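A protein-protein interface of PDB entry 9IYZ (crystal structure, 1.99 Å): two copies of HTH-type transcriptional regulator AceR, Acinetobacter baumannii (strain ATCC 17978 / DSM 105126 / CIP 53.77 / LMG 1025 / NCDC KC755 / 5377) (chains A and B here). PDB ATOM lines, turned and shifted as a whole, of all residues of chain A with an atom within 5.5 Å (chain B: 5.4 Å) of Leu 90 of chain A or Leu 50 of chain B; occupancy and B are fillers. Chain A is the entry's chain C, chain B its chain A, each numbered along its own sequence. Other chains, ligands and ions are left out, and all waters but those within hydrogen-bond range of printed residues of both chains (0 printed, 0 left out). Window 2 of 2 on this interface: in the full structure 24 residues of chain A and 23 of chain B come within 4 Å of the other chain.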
ATOM      1  N   GLN A  85      28.197  22.227 -11.823  1.00  0.00           N
ATOM      2  CA  GLN A  85      27.726  21.043 -12.530  1.00  0.00           C
ATOM      3  C   GLN A  85      27.598  19.865 -11.573  1.00  0.00           C
ATOM      4  O   GLN A  85      26.615  19.113 -11.626  1.00  0.00           O
ATOM      5  CB  GLN A  85      28.673  20.696 -13.682  1.00  0.00           C
ATOM      6  CG  GLN A  85      28.560  21.604 -14.896  1.00  0.00           C
ATOM      7  CD  GLN A  85      29.823  21.580 -15.763  1.00  0.00           C
ATOM      8  OE1 GLN A  85      30.625  20.647 -15.687  1.00  0.00           O
ATOM      9  NE2 GLN A  85      29.990  22.599 -16.603  1.00  0.00           N
ATOM     10  N   HIS A  86      28.588  19.691 -10.693  1.00  0.00           N
ATOM     11  CA  HIS A  86      28.514  18.637  -9.688  1.00  0.00           C
ATOM     12  C   HIS A  86      27.340  18.858  -8.742  1.00  0.00           C
ATOM     13  O   HIS A  86      26.680  17.898  -8.327  1.00  0.00           O
ATOM     14  CB  HIS A  86      29.827  18.572  -8.912  1.00  0.00           C
ATOM     15  CG  HIS A  86      30.926  17.874  -9.649  1.00  0.00           C
ATOM     16  ND1 HIS A  86      30.847  16.551 -10.027  1.00  0.00           N
ATOM     17  CD2 HIS A  86      32.123  18.323 -10.094  1.00  0.00           C
ATOM     18  CE1 HIS A  86      31.954  16.213 -10.666  1.00  0.00           C
ATOM     19  NE2 HIS A  86      32.743  17.270 -10.721  1.00  0.00           N
ATOM     20  N   ALA A  87      27.058  20.118  -8.394  1.00  0.00           N
ATOM     21  CA  ALA A  87      25.932  20.411  -7.514  1.00  0.00           C
ATOM     22  C   ALA A  87      24.602  20.149  -8.212  1.00  0.00           C
ATOM     23  O   ALA A  87      23.716  19.493  -7.653  1.00  0.00           O
ATOM     24  CB  ALA A  87      26.009  21.855  -7.029  1.00  0.00           C
ATOM     25  N   HIS A  88      24.447  20.657  -9.439  1.00  0.00           N
ATOM     26  CA  HIS A  88      23.231  20.423 -10.213  1.00  0.00           C
ATOM     27  C   HIS A  88      23.010  18.944 -10.513  1.00  0.00           C
ATOM     28  O   HIS A  88      21.886  18.548 -10.839  1.00  0.00           O
ATOM     29  CB  HIS A  88      23.289  21.206 -11.529  1.00  0.00           C
ATOM     30  CG  HIS A  88      22.950  22.659 -11.391  1.00  0.00           C
ATOM     31  ND1 HIS A  88      22.950  23.528 -12.462  1.00  0.00           N
ATOM     32  CD2 HIS A  88      22.605  23.396 -10.309  1.00  0.00           C
ATOM     33  CE1 HIS A  88      22.622  24.738 -12.045  1.00  0.00           C
ATOM     34  NE2 HIS A  88      22.407  24.687 -10.743  1.00  0.00           N
ATOM     35  N   ALA A  89      24.059  18.125 -10.418  1.00  0.00           N
ATOM     36  CA  ALA A  89      23.974  16.701 -10.708  1.00  0.00           C
ATOM     37  C   ALA A  89      23.483  15.874  -9.526  1.00  0.00           C
ATOM     38  O   ALA A  89      23.155  14.698  -9.711  1.00  0.00           O
ATOM     39  CB  ALA A  89      25.342  16.177 -11.154  1.00  0.00           C
ATOM     40  N   LEU A  90      23.420  16.450  -8.329  1.00  0.00           N
ATOM     41  CA  LEU A  90      23.067  15.688  -7.137  1.00  0.00           C
ATOM     42  C   LEU A  90      21.592  15.838  -6.794  1.00  0.00           C
ATOM     43  O   LEU A  90      21.044  15.056  -6.019  1.00  0.00           O
ATOM     44  CB  LEU A  90      23.919  16.137  -5.955  1.00  0.00           C
ATOM     45  CG  LEU A  90      25.427  15.943  -6.096  1.00  0.00           C
ATOM     46  CD1 LEU A  90      26.153  16.685  -4.978  1.00  0.00           C
ATOM     47  CD2 LEU A  90      25.787  14.463  -6.109  1.00  0.00           C
ATOM     48  OXT LEU A  90      20.921  16.756  -7.268  1.00  0.00           O
ATOM     49  N   LEU B  44      22.581  28.021   1.941  1.00  0.00           N
ATOM     50  CA  LEU B  44      23.285  27.192   0.965  1.00  0.00           C
ATOM     51  C   LEU B  44      22.400  26.050   0.470  1.00  0.00           C
ATOM     52  O   LEU B  44      22.343  25.772  -0.737  1.00  0.00           O
ATOM     53  CB  LEU B  44      24.573  26.649   1.583  1.00  0.00           C
ATOM     54  CG  LEU B  44      25.380  25.643   0.769  1.00  0.00           C
ATOM     55  CD1 LEU B  44      25.804  26.265  -0.566  1.00  0.00           C
ATOM     56  CD2 LEU B  44      26.588  25.183   1.574  1.00  0.00           C
ATOM     57  N   GLU B  45      21.711  25.370   1.397  1.00  0.00           N
ATOM     58  CA  GLU B  45      20.787  24.301   1.023  1.00  0.00           C
ATOM     59  C   GLU B  45      19.679  24.829   0.122  1.00  0.00           C
ATOM     60  O   GLU B  45      19.283  24.164  -0.842  1.00  0.00           O
ATOM     61  CB  GLU B  45      20.187  23.654   2.276  1.00  0.00           C
ATOM     62  CG  GLU B  45      21.199  22.900   3.147  1.00  0.00           C
ATOM     63  CD  GLU B  45      20.548  22.142   4.304  1.00  0.00           C
ATOM     64  OE1 GLU B  45      19.646  22.702   4.949  1.00  0.00           O
ATOM     65  OE2 GLU B  45      20.945  20.988   4.582  1.00  0.00           O
ATOM     66  N   ILE B  46      19.168  26.027   0.418  1.00  0.00           N
ATOM     67  CA  ILE B  46      18.158  26.633  -0.447  1.00  0.00           C
ATOM     68  C   ILE B  46      18.747  26.928  -1.823  1.00  0.00           C
ATOM     69  O   ILE B  46      18.156  26.583  -2.851  1.00  0.00           O
ATOM     70  CB  ILE B  46      17.569  27.895   0.209  1.00  0.00           C
ATOM     71  CG1 ILE B  46      16.817  27.516   1.478  1.00  0.00           C
ATOM     72  CG2 ILE B  46      16.598  28.585  -0.732  1.00  0.00           C
ATOM     73  CD1 ILE B  46      16.514  28.679   2.401  1.00  0.00           C
ATOM     74  N   LEU B  48      21.349  25.630  -3.460  1.00  0.00           N
ATOM     75  CA  LEU B  48      21.612  24.368  -4.150  1.00  0.00           C
ATOM     76  C   LEU B  48      20.373  23.510  -4.341  1.00  0.00           C
ATOM     77  O   LEU B  48      20.414  22.581  -5.155  1.00  0.00           O
ATOM     78  CB  LEU B  48      22.643  23.544  -3.375  1.00  0.00           C
ATOM     79  CG  LEU B  48      24.022  24.102  -3.071  1.00  0.00           C
ATOM     80  CD1 LEU B  48      24.870  23.069  -2.393  1.00  0.00           C
ATOM     81  CD2 LEU B  48      24.619  24.345  -4.420  1.00  0.00           C
ATOM     82  N   ASN B  49      19.292  23.789  -3.612  1.00  0.00           N
ATOM     83  CA  ASN B  49      18.152  22.882  -3.522  1.00  0.00           C
ATOM     84  C   ASN B  49      18.622  21.463  -3.213  1.00  0.00           C
ATOM     85  O   ASN B  49      18.301  20.499  -3.914  1.00  0.00           O
ATOM     86  CB  ASN B  49      17.307  22.919  -4.793  1.00  0.00           C
ATOM     87  CG  ASN B  49      15.898  22.432  -4.556  1.00  0.00           C
ATOM     88  OD1 ASN B  49      15.280  22.763  -3.538  1.00  0.00           O
ATOM     89  ND2 ASN B  49      15.377  21.641  -5.491  1.00  0.00           N
ATOM     90  N   LEU B  50      19.410  21.350  -2.146  1.00  0.00           N
ATOM     91  CA  LEU B  50      19.993  20.090  -1.701  1.00  0.00           C
ATOM     92  C   LEU B  50      19.955  20.085  -0.186  1.00  0.00           C
ATOM     93  O   LEU B  50      20.383  21.055   0.443  1.00  0.00           O
ATOM     94  CB  LEU B  50      21.446  19.947  -2.171  1.00  0.00           C
ATOM     95  CG  LEU B  50      21.782  19.207  -3.466  1.00  0.00           C
ATOM     96  CD1 LEU B  50      23.290  19.215  -3.682  1.00  0.00           C
ATOM     97  CD2 LEU B  50      21.250  17.785  -3.447  1.00  0.00           C
ATOM     98  N   THR B  51      19.447  19.014   0.405  1.00  0.00           N
ATOM     99  CA  THR B  51      19.540  18.876   1.849  1.00  0.00           C
ATOM    100  C   THR B  51      20.941  18.382   2.177  1.00  0.00           C
ATOM    101  O   THR B  51      21.367  17.347   1.659  1.00  0.00           O
ATOM    102  CB  THR B  51      18.468  17.926   2.369  1.00  0.00           C
ATOM    103  OG1 THR B  51      17.181  18.539   2.216  1.00  0.00           O
ATOM    104  CG2 THR B  51      18.699  17.612   3.840  1.00  0.00           C
ATOM    105  N   LEU B  52      21.680  19.137   2.996  1.00  0.00           N
ATOM    106  CA  LEU B  52      23.077  18.809   3.255  1.00  0.00           C
ATOM    107  C   LEU B  52      23.311  18.130   4.594  1.00  0.00           C
ATOM    108  O   LEU B  52      24.333  17.450   4.751  1.00  0.00           O
ATOM    109  CB  LEU B  52      23.958  20.067   3.160  1.00  0.00           C
ATOM    110  CG  LEU B  52      24.172  20.680   1.761  1.00  0.00           C
ATOM    111  CD1 LEU B  52      24.796  22.068   1.837  1.00  0.00           C
ATOM    112  CD2 LEU B  52      25.016  19.781   0.837  1.00  0.00           C
ATOM    113  N   GLU B  65      23.907  12.258   2.027  1.00  0.00           N
ATOM    114  CA  GLU B  65      24.561  11.564   0.922  1.00  0.00           C
ATOM    115  C   GLU B  65      25.182  12.567  -0.049  1.00  0.00           C
ATOM    116  O   GLU B  65      26.318  12.399  -0.503  1.00  0.00           O
ATOM    117  CB  GLU B  65      23.536  10.662   0.212  1.00  0.00           C
ATOM    118  CG  GLU B  65      23.019  11.121  -1.200  1.00  0.00           C
ATOM    119  CD  GLU B  65      22.063  12.337  -1.190  1.00  0.00           C
ATOM    120  OE1 GLU B  65      22.008  13.077  -0.183  1.00  0.00           O
ATOM    121  OE2 GLU B  65      21.374  12.564  -2.208  1.00  0.00           O
ATOM    122  N   ALA B  66      24.455  13.642  -0.350  1.00  0.00           N
ATOM    123  CA  ALA B  66      24.890  14.569  -1.380  1.00  0.00           C
ATOM    124  C   ALA B  66      25.974  15.508  -0.876  1.00  0.00           C
ATOM    125  O   ALA B  66      26.742  16.032  -1.686  1.00  0.00           O
ATOM    126  CB  ALA B  66      23.689  15.361  -1.909  1.00  0.00           C
ATOM    127  N   LEU B  69      29.645  16.480  -1.548  1.00  0.00           N
ATOM    128  CA  LEU B  69      30.060  17.693  -2.235  1.00  0.00           C
ATOM    129  C   LEU B  69      31.180  18.433  -1.507  1.00  0.00           C
ATOM    130  O   LEU B  69      31.777  19.344  -2.091  1.00  0.00           O
ATOM    131  CB  LEU B  69      28.830  18.600  -2.402  1.00  0.00           C
ATOM    132  CG  LEU B  69      28.889  19.798  -3.361  1.00  0.00           C
ATOM    133  CD1 LEU B  69      28.429  19.428  -4.764  1.00  0.00           C
ATOM    134  CD2 LEU B  69      28.056  20.947  -2.805  1.00  0.00           C
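O of Glu 45 of chain B lies within hydrogen-bond range of N of Leu 50 of chain B, 3.1 Å away.
CD2 of Leu 48 of chain B touches CB of Ala 87 of chain A, 3.9 Å away.
CD1 of Leu 69 of chain B touches CA of Ala 87 of chain A, 3.8 Å away.
Leu 90 of chain A touches Leu 50 of chain B (O to CD2, 3.8 Å).
Ala 66 of chain B touches Leu 90 of chain A (O to CD1, 3.4 Å).
CD1 of Leu 69 of chain B touches CD1 of Leu 90 of chain A, at 3.6 Å.
His 86 of chain A touches none of the printed residues of chain B.
Printed residues of chain B within 4 Å of Ala 87 of chain A: Leu 48 (3.9 Å) and Leu 69 (3.8 Å).
Of chain B, only Leu 50 (3.8 Å), Ala 66 (3.4 Å) and Leu 69 (3.6 Å) come within 4 Å of Leu 90 of chain A.
Glu 45 of chain B touches none of the printed residues of chain A.
Of the printed residues of chain A, Leu 48 of chain B touches Ala 87 (3.9 Å).
Of the printed residues of chain A, Ala 66 of chain B touches Leu 90 (3.4 Å).
Of the printed residues of chain A, Leu 69 of chain B touches Ala 87 and Leu 90.
Hydrophobic or aromatic side chains of chain A that line the printed part of chain B: Ala 87 and Leu 90.
Of the 11 printed residues of chain B, 4 touch a printed residue of chain A.
No position is printed for both chains.
Of the 5 pairs that touch across the chains among the printed residues, none has its exchanged pair printed and touching as well.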
